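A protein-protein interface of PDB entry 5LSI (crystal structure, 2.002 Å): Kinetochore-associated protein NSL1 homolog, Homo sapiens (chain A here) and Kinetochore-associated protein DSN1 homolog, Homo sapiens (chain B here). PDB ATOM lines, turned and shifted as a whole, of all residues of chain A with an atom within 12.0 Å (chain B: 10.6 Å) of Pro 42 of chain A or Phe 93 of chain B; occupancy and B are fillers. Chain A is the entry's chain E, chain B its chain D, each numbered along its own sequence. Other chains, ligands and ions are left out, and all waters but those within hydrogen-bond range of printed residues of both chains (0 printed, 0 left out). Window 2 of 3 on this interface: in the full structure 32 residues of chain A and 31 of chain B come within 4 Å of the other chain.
The backbone carbonyl oxygen (O) of Gly 38 of chain A lies within hydrogen-bond range of the guanidinium group (NE) of Arg 46 of chain A, at 2.9 Å.
O of Leu 41 of chain A sits at hydrogen-bond distance from NH2 of Arg 46 of chain A.
Printed residues of chain B within 4 Å of Lys 36 of chain A: Lys 101.
Of the printed residues of chain B, Asp 39 of chain A touches Phe 93 (3.4 Å) and Lys 101 (2.5 Å).
Ala 40 of chain A touches just these residues of chain B: Phe 93 (3.3 Å), Phe 98 (3.6 Å) and Lys 101 (3.9 Å).
Of chain B, only Leu 87 (3.9 Å), Phe 93 (3.1 Å) and Phe 98 (3.6 Å) come within 4 Å of Leu 41 of chain A.
Of the printed residues of chain A, Leu 83 of chain B touches Ala 49 (3.8 Å).
Leu 87 of chain B touches just these residues of chain A: Leu 41 (3.9 Å) and Ile 45 (3.8 Å).
No residue of chain A comes within 4 Å of Asp 89 of chain B.
Thr 90 of chain B touches none of the printed residues of chain A.
No residue of chain A comes within 4 Å of Gly 92 of chain B.
Printed residues of chain A within 4 Å of Phe 93 of chain B: Asp 39 (3.4 Å), Ala 40 (3.3 Å), Leu 41 (3.1 Å), Pro 42 (3.6 Å) and Arg 46 (3.7 Å).
No residue of chain A comes within 4 Å of Ser 94 of chain B.
No residue of chain A comes within 4 Å of Ser 97 of chain B.
Of the printed residues of chain A, Phe 98 of chain B touches Ala 40 and Leu 41.
Of the printed residues of chain A, Lys 101 of chain B touches Lys 36 (3.0 Å), Asp 39 (2.5 Å) and Ala 40 (3.9 Å).
The nearest residue of chain B that does not touch Pro 42 of chain A is Thr 90 of chain B (4.5 Å).
The side-chain amino group (NZ) of Lys 101 of chain B lies within hydrogen-bond range of the backbone carbonyl oxygen (O) of Lys 36 of chain A.
The side-chain amino group (NZ) of Lys 101 of chain B is in salt-bridge range of the side-chain carboxylate (OD2) of Asp 39 of chain A (2.5 Å).
Among the printed residues, pairs that only touch across the chains: Leu 41 of chain A with Phe 93 of chain B (3.1 Å), Ala 40 of chain A with Phe 93 of chain B (3.3 Å), Asp 39 of chain A with Phe 93 of chain B (3.4 Å), Leu 41 of chain A with Phe 98 of chain B (3.6 Å), Ala 40 of chain A with Phe 98 of chain B (3.6 Å), Pro 42 of chain A with Phe 93 of chain B (3.6 Å), Arg 46 of chain A with Phe 93 of chain B (3.7 Å), Ala 49 of chain A with Leu 83 of chain B (3.8 Å), Ile 45 of chain A with Leu 87 of chain B (3.8 Å), Leu 41 of chain A with Leu 87 of chain B (3.9 Å) and Ala 40 of chain A with Lys 101 of chain B (3.9 Å).
Hydrophobic or aromatic side chains of chain B that line the printed part of chain A: Leu 83, Leu 87, Phe 93 and Phe 98.
Printed residues of chain A that touch a printed residue of chain B: Lys 36, Asp 39, Ala 40, Leu 41, Pro 42, Ile 45, Arg 46 and Ala 49.
Hydrophobic or aromatic side chains of chain A within 4 Å of the printed part of chain B: Ala 40, Leu 41, Pro 42, Ile 45 and Ala 49.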
ATOM      1  N   VAL A  34     -17.137 -11.146  23.816  1.00  0.00           N
ATOM      2  CA  VAL A  34     -18.281 -12.048  23.735  1.00  0.00           C
ATOM      3  C   VAL A  34     -19.401 -11.414  22.916  1.00  0.00           C
ATOM      4  O   VAL A  34     -20.066 -12.091  22.122  1.00  0.00           O
ATOM      5  CB  VAL A  34     -18.761 -12.435  25.144  1.00  0.00           C
ATOM      6  CG1 VAL A  34     -19.978 -13.343  25.058  1.00  0.00           C
ATOM      7  CG2 VAL A  34     -17.639 -13.112  25.916  1.00  0.00           C
ATOM      8  N   GLN A  35     -19.626 -10.107  23.095  1.00  0.00           N
ATOM      9  CA  GLN A  35     -20.673  -9.419  22.345  1.00  0.00           C
ATOM     10  C   GLN A  35     -20.399  -9.454  20.847  1.00  0.00           C
ATOM     11  O   GLN A  35     -21.330  -9.571  20.044  1.00  0.00           O
ATOM     12  CB  GLN A  35     -20.801  -7.974  22.829  1.00  0.00           C
ATOM     13  CG  GLN A  35     -21.196  -7.841  24.287  1.00  0.00           C
ATOM     14  CD  GLN A  35     -22.634  -8.242  24.536  1.00  0.00           C
ATOM     15  OE1 GLN A  35     -22.933  -8.972  25.481  1.00  0.00           O
ATOM     16  NE2 GLN A  35     -23.538  -7.759  23.689  1.00  0.00           N
ATOM     17  N   LYS A  36     -19.126  -9.361  20.453  1.00  0.00           N
ATOM     18  CA  LYS A  36     -18.782  -9.381  19.035  1.00  0.00           C
ATOM     19  C   LYS A  36     -19.150 -10.699  18.367  1.00  0.00           C
ATOM     20  O   LYS A  36     -19.250 -10.748  17.137  1.00  0.00           O
ATOM     21  CB  LYS A  36     -17.289  -9.106  18.846  1.00  0.00           C
ATOM     22  CG  LYS A  36     -16.806  -7.812  19.472  1.00  0.00           C
ATOM     23  CD  LYS A  36     -17.595  -6.613  18.983  1.00  0.00           C
ATOM     24  CE  LYS A  36     -16.689  -5.615  18.276  1.00  0.00           C
ATOM     25  NZ  LYS A  36     -17.440  -4.434  17.762  1.00  0.00           N
ATOM     26  N   LEU A  37     -19.343 -11.768  19.142  1.00  0.00           N
ATOM     27  CA  LEU A  37     -19.811 -13.027  18.572  1.00  0.00           C
ATOM     28  C   LEU A  37     -21.217 -12.918  18.006  1.00  0.00           C
ATOM     29  O   LEU A  37     -21.580 -13.722  17.141  1.00  0.00           O
ATOM     30  CB  LEU A  37     -19.792 -14.128  19.624  1.00  0.00           C
ATOM     31  CG  LEU A  37     -18.432 -14.613  20.099  1.00  0.00           C
ATOM     32  CD1 LEU A  37     -18.605 -15.214  21.478  1.00  0.00           C
ATOM     33  CD2 LEU A  37     -17.876 -15.635  19.121  1.00  0.00           C
ATOM     34  N   GLY A  38     -22.012 -11.953  18.482  1.00  0.00           N
ATOM     35  CA  GLY A  38     -23.379 -11.827  18.013  1.00  0.00           C
ATOM     36  C   GLY A  38     -23.475 -11.625  16.515  1.00  0.00           C
ATOM     37  O   GLY A  38     -24.493 -11.958  15.908  1.00  0.00           O
ATOM     38  N   ASP A  39     -22.421 -11.080  15.902  1.00  0.00           N
ATOM     39  CA  ASP A  39     -22.399 -10.933  14.450  1.00  0.00           C
ATOM     40  C   ASP A  39     -22.590 -12.280  13.765  1.00  0.00           C
ATOM     41  O   ASP A  39     -23.432 -12.419  12.871  1.00  0.00           O
ATOM     42  CB  ASP A  39     -21.086 -10.287  14.007  1.00  0.00           C
ATOM     43  CG  ASP A  39     -20.737  -9.040  14.818  1.00  0.00           C
ATOM     44  OD1 ASP A  39     -21.658  -8.260  15.153  1.00  0.00           O
ATOM     45  OD2 ASP A  39     -19.533  -8.838  15.106  1.00  0.00           O
ATOM     46  N   ALA A  40     -21.836 -13.292  14.195  1.00  0.00           N
ATOM     47  CA  ALA A  40     -21.926 -14.618  13.599  1.00  0.00           C
ATOM     48  C   ALA A  40     -23.117 -15.425  14.104  1.00  0.00           C
ATOM     49  O   ALA A  40     -23.346 -16.533  13.607  1.00  0.00           O
ATOM     50  CB  ALA A  40     -20.636 -15.398  13.858  1.00  0.00           C
ATOM     51  N   LEU A  41     -23.876 -14.906  15.069  1.00  0.00           N
ATOM     52  CA  LEU A  41     -25.010 -15.671  15.573  1.00  0.00           C
ATOM     53  C   LEU A  41     -26.285 -15.292  14.824  1.00  0.00           C
ATOM     54  O   LEU A  41     -26.470 -14.125  14.465  1.00  0.00           O
ATOM     55  CB  LEU A  41     -25.211 -15.427  17.065  1.00  0.00           C
ATOM     56  CG  LEU A  41     -24.200 -16.086  18.002  1.00  0.00           C
ATOM     57  CD1 LEU A  41     -24.573 -15.829  19.455  1.00  0.00           C
ATOM     58  CD2 LEU A  41     -24.116 -17.575  17.718  1.00  0.00           C
ATOM     59  N   PRO A  42     -27.177 -16.248  14.585  1.00  0.00           N
ATOM     60  CA  PRO A  42     -28.440 -15.926  13.918  1.00  0.00           C
ATOM     61  C   PRO A  42     -29.392 -15.206  14.859  1.00  0.00           C
ATOM     62  O   PRO A  42     -29.392 -15.420  16.073  1.00  0.00           O
ATOM     63  CB  PRO A  42     -28.995 -17.298  13.506  1.00  0.00           C
ATOM     64  CG  PRO A  42     -27.986 -18.324  13.982  1.00  0.00           C
ATOM     65  CD  PRO A  42     -27.121 -17.658  14.995  1.00  0.00           C
ATOM     66  N   GLU A  43     -30.212 -14.334  14.265  1.00  0.00           N
ATOM     67  CA  GLU A  43     -31.130 -13.508  15.044  1.00  0.00           C
ATOM     68  C   GLU A  43     -32.076 -14.351  15.892  1.00  0.00           C
ATOM     69  O   GLU A  43     -32.568 -13.881  16.926  1.00  0.00           O
ATOM     70  CB  GLU A  43     -31.913 -12.596  14.099  1.00  0.00           C
ATOM     71  CG  GLU A  43     -32.942 -11.703  14.764  1.00  0.00           C
ATOM     72  CD  GLU A  43     -33.614 -10.772  13.778  1.00  0.00           C
ATOM     73  OE1 GLU A  43     -32.891 -10.080  13.030  1.00  0.00           O
ATOM     74  OE2 GLU A  43     -34.863 -10.741  13.741  1.00  0.00           O
ATOM     75  N   GLU A  44     -32.315 -15.601  15.485  1.00  0.00           N
ATOM     76  CA  GLU A  44     -33.264 -16.464  16.183  1.00  0.00           C
ATOM     77  C   GLU A  44     -32.853 -16.697  17.633  1.00  0.00           C
ATOM     78  O   GLU A  44     -33.701 -16.698  18.534  1.00  0.00           O
ATOM     79  CB  GLU A  44     -33.386 -17.796  15.435  1.00  0.00           C
ATOM     80  CG  GLU A  44     -34.653 -18.580  15.737  1.00  0.00           C
ATOM     81  CD  GLU A  44     -34.748 -19.869  14.930  1.00  0.00           C
ATOM     82  OE1 GLU A  44     -35.416 -20.819  15.397  1.00  0.00           O
ATOM     83  OE2 GLU A  44     -34.156 -19.935  13.829  1.00  0.00           O
ATOM     84  N   ILE A  45     -31.560 -16.912  17.876  1.00  0.00           N
ATOM     85  CA  ILE A  45     -31.050 -17.285  19.186  1.00  0.00           C
ATOM     86  C   ILE A  45     -30.041 -16.277  19.721  1.00  0.00           C
ATOM     87  O   ILE A  45     -29.454 -16.503  20.780  1.00  0.00           O
ATOM     88  CB  ILE A  45     -30.429 -18.696  19.159  1.00  0.00           C
ATOM     89  CG1 ILE A  45     -29.368 -18.774  18.058  1.00  0.00           C
ATOM     90  CG2 ILE A  45     -31.507 -19.749  18.962  1.00  0.00           C
ATOM     91  CD1 ILE A  45     -28.232 -19.730  18.358  1.00  0.00           C
ATOM     92  N   ARG A  46     -29.834 -15.162  19.013  1.00  0.00           N
ATOM     93  CA  ARG A  46     -28.705 -14.281  19.313  1.00  0.00           C
ATOM     94  C   ARG A  46     -28.736 -13.787  20.756  1.00  0.00           C
ATOM     95  O   ARG A  46     -27.756 -13.940  21.493  1.00  0.00           O
ATOM     96  CB  ARG A  46     -28.683 -13.100  18.342  1.00  0.00           C
ATOM     97  CG  ARG A  46     -27.535 -12.132  18.593  1.00  0.00           C
ATOM     98  CD  ARG A  46     -27.472 -11.027  17.547  1.00  0.00           C
ATOM     99  NE  ARG A  46     -27.311 -11.560  16.197  1.00  0.00           N
ATOM    100  CZ  ARG A  46     -28.114 -11.271  15.176  1.00  0.00           C
ATOM    101  NH1 ARG A  46     -29.136 -10.444  15.346  1.00  0.00           N
ATOM    102  NH2 ARG A  46     -27.891 -11.805  13.982  1.00  0.00           N
ATOM    103  N   GLU A  47     -29.852 -13.192  21.180  1.00  0.00           N
ATOM    104  CA  GLU A  47     -29.909 -12.616  22.522  1.00  0.00           C
ATOM    105  C   GLU A  47     -29.726 -13.651  23.627  1.00  0.00           C
ATOM    106  O   GLU A  47     -28.854 -13.448  24.487  1.00  0.00           O
ATOM    107  CB  GLU A  47     -31.214 -11.833  22.705  1.00  0.00           C
ATOM    108  CG  GLU A  47     -31.266 -10.519  21.960  1.00  0.00           C
ATOM    109  CD  GLU A  47     -32.434  -9.662  22.402  1.00  0.00           C
ATOM    110  OE1 GLU A  47     -33.466 -10.235  22.819  1.00  0.00           O
ATOM    111  OE2 GLU A  47     -32.317  -8.418  22.345  1.00  0.00           O
ATOM    112  N   PRO A  48     -30.488 -14.752  23.683  1.00  0.00           N
ATOM    113  CA  PRO A  48     -30.246 -15.723  24.761  1.00  0.00           C
ATOM    114  C   PRO A  48     -28.884 -16.392  24.671  1.00  0.00           C
ATOM    115  O   PRO A  48     -28.300 -16.711  25.714  1.00  0.00           O
ATOM    116  CB  PRO A  48     -31.388 -16.733  24.587  1.00  0.00           C
ATOM    117  CG  PRO A  48     -31.755 -16.631  23.154  1.00  0.00           C
ATOM    118  CD  PRO A  48     -31.598 -15.182  22.813  1.00  0.00           C
ATOM    119  N   ALA A  49     -28.354 -16.601  23.461  1.00  0.00           N
ATOM    120  CA  ALA A  49     -27.040 -17.223  23.324  1.00  0.00           C
ATOM    121  C   ALA A  49     -25.937 -16.320  23.860  1.00  0.00           C
ATOM    122  O   ALA A  49     -24.966 -16.803  24.455  1.00  0.00           O
ATOM    123  CB  ALA A  49     -26.773 -17.582  21.864  1.00  0.00           C
ATOM    124  N   LEU A  50     -26.067 -15.005  23.663  1.00  0.00           N
ATOM    125  CA  LEU A  50     -25.051 -14.085  24.161  1.00  0.00           C
ATOM    126  C   LEU A  50     -25.106 -13.971  25.679  1.00  0.00           C
ATOM    127  O   LEU A  50     -24.062 -13.915  26.338  1.00  0.00           O
ATOM    128  CB  LEU A  50     -25.213 -12.710  23.513  1.00  0.00           C
ATOM    129  CG  LEU A  50     -24.678 -12.566  22.086  1.00  0.00           C
ATOM    130  CD1 LEU A  50     -24.776 -11.123  21.616  1.00  0.00           C
ATOM    131  CD2 LEU A  50     -23.241 -13.063  22.001  1.00  0.00           C
ATOM    132  N   ARG A  51     -26.312 -13.915  26.253  1.00  0.00           N
ATOM    133  CA  ARG A  51     -26.425 -13.968  27.707  1.00  0.00           C
ATOM    134  C   ARG A  51     -25.810 -15.249  28.252  1.00  0.00           C
ATOM    135  O   ARG A  51     -25.083 -15.224  29.254  1.00  0.00           O
ATOM    136  CB  ARG A  51     -27.890 -13.857  28.133  1.00  0.00           C
ATOM    137  CG  ARG A  51     -28.499 -12.468  27.960  1.00  0.00           C
ATOM    138  CD  ARG A  51     -29.814 -12.338  28.729  1.00  0.00           C
ATOM    139  NE  ARG A  51     -30.809 -13.319  28.302  1.00  0.00           N
ATOM    140  CZ  ARG A  51     -31.701 -13.110  27.340  1.00  0.00           C
ATOM    141  NH1 ARG A  51     -31.729 -11.948  26.701  1.00  0.00           N
ATOM    142  NH2 ARG A  51     -32.564 -14.063  27.019  1.00  0.00           N
ATOM    143  N   ALA A  53     -23.481 -17.188  26.787  1.00  0.00           N
ATOM    144  CA  ALA A  53     -22.032 -17.166  26.587  1.00  0.00           C
ATOM    145  C   ALA A  53     -21.344 -16.234  27.575  1.00  0.00           C
ATOM    146  O   ALA A  53     -20.274 -16.556  28.102  1.00  0.00           O
ATOM    147  CB  ALA A  53     -21.703 -16.755  25.152  1.00  0.00           C
ATOM    148  N   LEU B  83     -21.157 -23.362  23.205  1.00  0.00           N
ATOM    149  CA  LEU B  83     -22.176 -22.778  22.345  1.00  0.00           C
ATOM    150  C   LEU B  83     -22.185 -23.381  20.947  1.00  0.00           C
ATOM    151  O   LEU B  83     -23.252 -23.470  20.326  1.00  0.00           O
ATOM    152  CB  LEU B  83     -21.958 -21.264  22.255  1.00  0.00           C
ATOM    153  CG  LEU B  83     -22.901 -20.431  21.393  1.00  0.00           C
ATOM    154  CD1 LEU B  83     -24.294 -20.422  21.992  1.00  0.00           C
ATOM    155  CD2 LEU B  83     -22.366 -19.015  21.245  1.00  0.00           C
ATOM    156  N   GLU B  84     -21.026 -23.814  20.454  1.00  0.00           N
ATOM    157  CA  GLU B  84     -20.914 -24.261  19.067  1.00  0.00           C
ATOM    158  C   GLU B  84     -21.805 -25.450  18.702  1.00  0.00           C
ATOM    159  O   GLU B  84     -22.349 -25.446  17.584  1.00  0.00           O
ATOM    160  CB  GLU B  84     -19.448 -24.581  18.755  1.00  0.00           C
ATOM    161  CG  GLU B  84     -19.159 -24.774  17.280  1.00  0.00           C
ATOM    162  CD  GLU B  84     -17.985 -25.700  17.034  1.00  0.00           C
ATOM    163  OE1 GLU B  84     -18.220 -26.871  16.658  1.00  0.00           O
ATOM    164  OE2 GLU B  84     -16.830 -25.264  17.225  1.00  0.00           O
ATOM    165  N   PHE B  86     -24.710 -26.019  19.233  1.00  0.00           N
ATOM    166  CA  PHE B  86     -26.088 -25.577  19.070  1.00  0.00           C
ATOM    167  C   PHE B  86     -26.260 -24.620  17.894  1.00  0.00           C
ATOM    168  O   PHE B  86     -27.249 -23.882  17.843  1.00  0.00           O
ATOM    169  CB  PHE B  86     -26.577 -24.926  20.363  1.00  0.00           C
ATOM    170  CG  PHE B  86     -26.355 -25.776  21.579  1.00  0.00           C
ATOM    171  CD1 PHE B  86     -26.704 -27.116  21.573  1.00  0.00           C
ATOM    172  CD2 PHE B  86     -25.778 -25.243  22.719  1.00  0.00           C
ATOM    173  CE1 PHE B  86     -26.496 -27.907  22.685  1.00  0.00           C
ATOM    174  CE2 PHE B  86     -25.568 -26.030  23.837  1.00  0.00           C
ATOM    175  CZ  PHE B  86     -25.927 -27.364  23.819  1.00  0.00           C
ATOM    176  N   LEU B  87     -25.320 -24.621  16.953  1.00  0.00           N
ATOM    177  CA  LEU B  87     -25.360 -23.761  15.777  1.00  0.00           C
ATOM    178  C   LEU B  87     -25.428 -24.632  14.532  1.00  0.00           C
ATOM    179  O   LEU B  87     -24.647 -25.578  14.391  1.00  0.00           O
ATOM    180  CB  LEU B  87     -24.127 -22.855  15.719  1.00  0.00           C
ATOM    181  CG  LEU B  87     -23.737 -22.111  16.998  1.00  0.00           C
ATOM    182  CD1 LEU B  87     -22.634 -21.127  16.715  1.00  0.00           C
ATOM    183  CD2 LEU B  87     -24.912 -21.385  17.610  1.00  0.00           C
ATOM    184  N   ARG B  88     -26.348 -24.311  13.624  1.00  0.00           N
ATOM    185  CA  ARG B  88     -26.518 -25.084  12.403  1.00  0.00           C
ATOM    186  C   ARG B  88     -26.457 -24.158  11.193  1.00  0.00           C
ATOM    187  O   ARG B  88     -26.575 -22.935  11.311  1.00  0.00           O
ATOM    188  CB  ARG B  88     -27.827 -25.884  12.438  1.00  0.00           C
ATOM    189  CG  ARG B  88     -27.810 -26.969  13.510  1.00  0.00           C
ATOM    190  CD  ARG B  88     -29.198 -27.466  13.865  1.00  0.00           C
ATOM    191  NE  ARG B  88     -29.821 -28.194  12.765  1.00  0.00           N
ATOM    192  CZ  ARG B  88     -30.982 -28.831  12.859  1.00  0.00           C
ATOM    193  NH1 ARG B  88     -31.645 -28.834  14.008  1.00  0.00           N
ATOM    194  NH2 ARG B  88     -31.479 -29.470  11.808  1.00  0.00           N
ATOM    195  N   ASP B  89     -26.263 -24.764  10.021  1.00  0.00           N
ATOM    196  CA  ASP B  89     -25.933 -24.041   8.791  1.00  0.00           C
ATOM    197  C   ASP B  89     -27.126 -23.353   8.136  1.00  0.00           C
ATOM    198  O   ASP B  89     -27.302 -23.460   6.919  1.00  0.00           O
ATOM    199  CB  ASP B  89     -25.273 -25.008   7.810  1.00  0.00           C
ATOM    200  CG  ASP B  89     -23.759 -24.979   7.888  1.00  0.00           C
ATOM    201  OD1 ASP B  89     -23.158 -23.992   7.417  1.00  0.00           O
ATOM    202  OD2 ASP B  89     -23.169 -25.945   8.415  1.00  0.00           O
ATOM    203  N   THR B  90     -27.953 -22.640   8.898  1.00  0.00           N
ATOM    204  CA  THR B  90     -29.040 -21.890   8.288  1.00  0.00           C
ATOM    205  C   THR B  90     -28.477 -20.799   7.379  1.00  0.00           C
ATOM    206  O   THR B  90     -27.341 -20.342   7.542  1.00  0.00           O
ATOM    207  CB  THR B  90     -29.948 -21.275   9.354  1.00  0.00           C
ATOM    208  OG1 THR B  90     -29.242 -20.239  10.048  1.00  0.00           O
ATOM    209  CG2 THR B  90     -30.400 -22.335  10.349  1.00  0.00           C
ATOM    210  N   LYS B  91     -29.288 -20.388   6.405  1.00  0.00           N
ATOM    211  CA  LYS B  91     -28.820 -19.459   5.382  1.00  0.00           C
ATOM    212  C   LYS B  91     -28.381 -18.142   6.010  1.00  0.00           C
ATOM    213  O   LYS B  91     -29.084 -17.570   6.848  1.00  0.00           O
ATOM    214  CB  LYS B  91     -29.917 -19.218   4.342  1.00  0.00           C
ATOM    215  CG  LYS B  91     -29.392 -18.779   2.978  1.00  0.00           C
ATOM    216  CD  LYS B  91     -30.494 -18.771   1.923  1.00  0.00           C
ATOM    217  CE  LYS B  91     -30.401 -19.989   1.013  1.00  0.00           C
ATOM    218  NZ  LYS B  91     -30.830 -19.693  -0.384  1.00  0.00           N
ATOM    219  N   GLY B  92     -27.202 -17.672   5.606  1.00  0.00           N
ATOM    220  CA  GLY B  92     -26.622 -16.468   6.154  1.00  0.00           C
ATOM    221  C   GLY B  92     -25.799 -16.667   7.408  1.00  0.00           C
ATOM    222  O   GLY B  92     -25.168 -15.707   7.873  1.00  0.00           O
ATOM    223  N   PHE B  93     -25.779 -17.883   7.977  1.00  0.00           N
ATOM    224  CA  PHE B  93     -25.041 -18.164   9.212  1.00  0.00           C
ATOM    225  C   PHE B  93     -24.476 -19.583   9.126  1.00  0.00           C
ATOM    226  O   PHE B  93     -25.049 -20.544   9.647  1.00  0.00           O
ATOM    227  CB  PHE B  93     -25.926 -17.975  10.444  1.00  0.00           C
ATOM    228  CG  PHE B  93     -26.360 -16.552  10.661  1.00  0.00           C
ATOM    229  CD1 PHE B  93     -25.493 -15.631  11.228  1.00  0.00           C
ATOM    230  CD2 PHE B  93     -27.628 -16.135  10.290  1.00  0.00           C
ATOM    231  CE1 PHE B  93     -25.885 -14.320  11.424  1.00  0.00           C
ATOM    232  CE2 PHE B  93     -28.026 -14.824  10.486  1.00  0.00           C
ATOM    233  CZ  PHE B  93     -27.154 -13.916  11.054  1.00  0.00           C
ATOM    234  N   SER B  94     -23.333 -19.710   8.458  1.00  0.00           N
ATOM    235  CA  SER B  94     -22.630 -20.980   8.391  1.00  0.00           C
ATOM    236  C   SER B  94     -21.760 -21.160   9.625  1.00  0.00           C
ATOM    237  O   SER B  94     -21.171 -20.201  10.131  1.00  0.00           O
ATOM    238  CB  SER B  94     -21.765 -21.049   7.132  1.00  0.00           C
ATOM    239  OG  SER B  94     -20.619 -20.224   7.260  1.00  0.00           O
ATOM    240  N   LEU B  95     -21.684 -22.400  10.113  1.00  0.00           N
ATOM    241  CA  LEU B  95     -20.798 -22.684  11.237  1.00  0.00           C
ATOM    242  C   LEU B  95     -19.351 -22.377  10.875  1.00  0.00           C
ATOM    243  O   LEU B  95     -18.566 -21.971  11.740  1.00  0.00           O
ATOM    244  CB  LEU B  95     -20.970 -24.139  11.681  1.00  0.00           C
ATOM    245  CG  LEU B  95     -20.454 -24.601  13.051  1.00  0.00           C
ATOM    246  CD1 LEU B  95     -21.188 -25.851  13.501  1.00  0.00           C
ATOM    247  CD2 LEU B  95     -18.947 -24.815  13.100  1.00  0.00           C
ATOM    248  N   GLU B  96     -18.988 -22.545   9.601  1.00  0.00           N
ATOM    249  CA  GLU B  96     -17.667 -22.136   9.133  1.00  0.00           C
ATOM    250  C   GLU B  96     -17.410 -20.662   9.431  1.00  0.00           C
ATOM    251  O   GLU B  96     -16.339 -20.294   9.925  1.00  0.00           O
ATOM    252  CB  GLU B  96     -17.542 -22.413   7.635  1.00  0.00           C
ATOM    253  CG  GLU B  96     -16.649 -21.432   6.897  1.00  0.00           C
ATOM    254  CD  GLU B  96     -16.880 -21.449   5.398  1.00  0.00           C
ATOM    255  OE1 GLU B  96     -17.369 -22.478   4.883  1.00  0.00           O
ATOM    256  OE2 GLU B  96     -16.586 -20.428   4.739  1.00  0.00           O
ATOM    257  N   SER B  97     -18.389 -19.800   9.141  1.00  0.00           N
ATOM    258  CA  SER B  97     -18.208 -18.378   9.403  1.00  0.00           C
ATOM    259  C   SER B  97     -18.188 -18.081  10.898  1.00  0.00           C
ATOM    260  O   SER B  97     -17.519 -17.134  11.329  1.00  0.00           O
ATOM    261  CB  SER B  97     -19.303 -17.568   8.708  1.00  0.00           C
ATOM    262  OG  SER B  97     -20.593 -18.017   9.086  1.00  0.00           O
ATOM    263  N   PHE B  98     -18.906 -18.872  11.701  1.00  0.00           N
ATOM    264  CA  PHE B  98     -18.859 -18.686  13.149  1.00  0.00           C
ATOM    265  C   PHE B  98     -17.481 -19.021  13.701  1.00  0.00           C
ATOM    266  O   PHE B  98     -16.949 -18.289  14.543  1.00  0.00           O
ATOM    267  CB  PHE B  98     -19.927 -19.539  13.830  1.00  0.00           C
ATOM    268  CG  PHE B  98     -19.936 -19.413  15.329  1.00  0.00           C
ATOM    269  CD1 PHE B  98     -20.599 -18.363  15.945  1.00  0.00           C
ATOM    270  CD2 PHE B  98     -19.279 -20.342  16.122  1.00  0.00           C
ATOM    271  CE1 PHE B  98     -20.607 -18.243  17.325  1.00  0.00           C
ATOM    272  CE2 PHE B  98     -19.283 -20.225  17.501  1.00  0.00           C
ATOM    273  CZ  PHE B  98     -19.947 -19.175  18.103  1.00  0.00           C
ATOM    274  N   ARG B  99     -16.888 -20.127  13.243  1.00  0.00           N
ATOM    275  CA  ARG B  99     -15.545 -20.482  13.687  1.00  0.00           C
ATOM    276  C   ARG B  99     -14.518 -19.458  13.235  1.00  0.00           C
ATOM    277  O   ARG B  99     -13.536 -19.212  13.943  1.00  0.00           O
ATOM    278  CB  ARG B  99     -15.167 -21.867  13.172  1.00  0.00           C
ATOM    279  CG  ARG B  99     -15.996 -22.977  13.761  1.00  0.00           C
ATOM    280  CD  ARG B  99     -15.346 -24.320  13.529  1.00  0.00           C
ATOM    281  NE  ARG B  99     -15.730 -25.275  14.560  1.00  0.00           N
ATOM    282  CZ  ARG B  99     -15.139 -26.450  14.742  1.00  0.00           C
ATOM    283  NH1 ARG B  99     -14.136 -26.816  13.954  1.00  0.00           N
ATOM    284  NH2 ARG B  99     -15.553 -27.262  15.706  1.00  0.00           N
ATOM    285  N   ALA B 100     -14.718 -18.863  12.057  1.00  0.00           N
ATOM    286  CA  ALA B 100     -13.817 -17.808  11.606  1.00  0.00           C
ATOM    287  C   ALA B 100     -13.931 -16.576  12.493  1.00  0.00           C
ATOM    288  O   ALA B 100     -12.916 -15.961  12.843  1.00  0.00           O
ATOM    289  CB  ALA B 100     -14.111 -17.454  10.149  1.00  0.00           C
ATOM    290  N   LYS B 101     -15.155 -16.201  12.867  1.00  0.00           N
ATOM    291  CA  LYS B 101     -15.337 -15.055  13.750  1.00  0.00           C
ATOM    292  C   LYS B 101     -14.831 -15.358  15.154  1.00  0.00           C
ATOM    293  O   LYS B 101     -14.207 -14.504  15.794  1.00  0.00           O
ATOM    294  CB  LYS B 101     -16.810 -14.650  13.787  1.00  0.00           C
ATOM    295  CG  LYS B 101     -17.066 -13.276  14.390  1.00  0.00           C
ATOM    296  CD  LYS B 101     -16.277 -12.202  13.658  1.00  0.00           C
ATOM    297  CE  LYS B 101     -17.138 -10.985  13.360  1.00  0.00           C
ATOM    298  NZ  LYS B 101     -17.654 -10.349  14.603  1.00  0.00           N
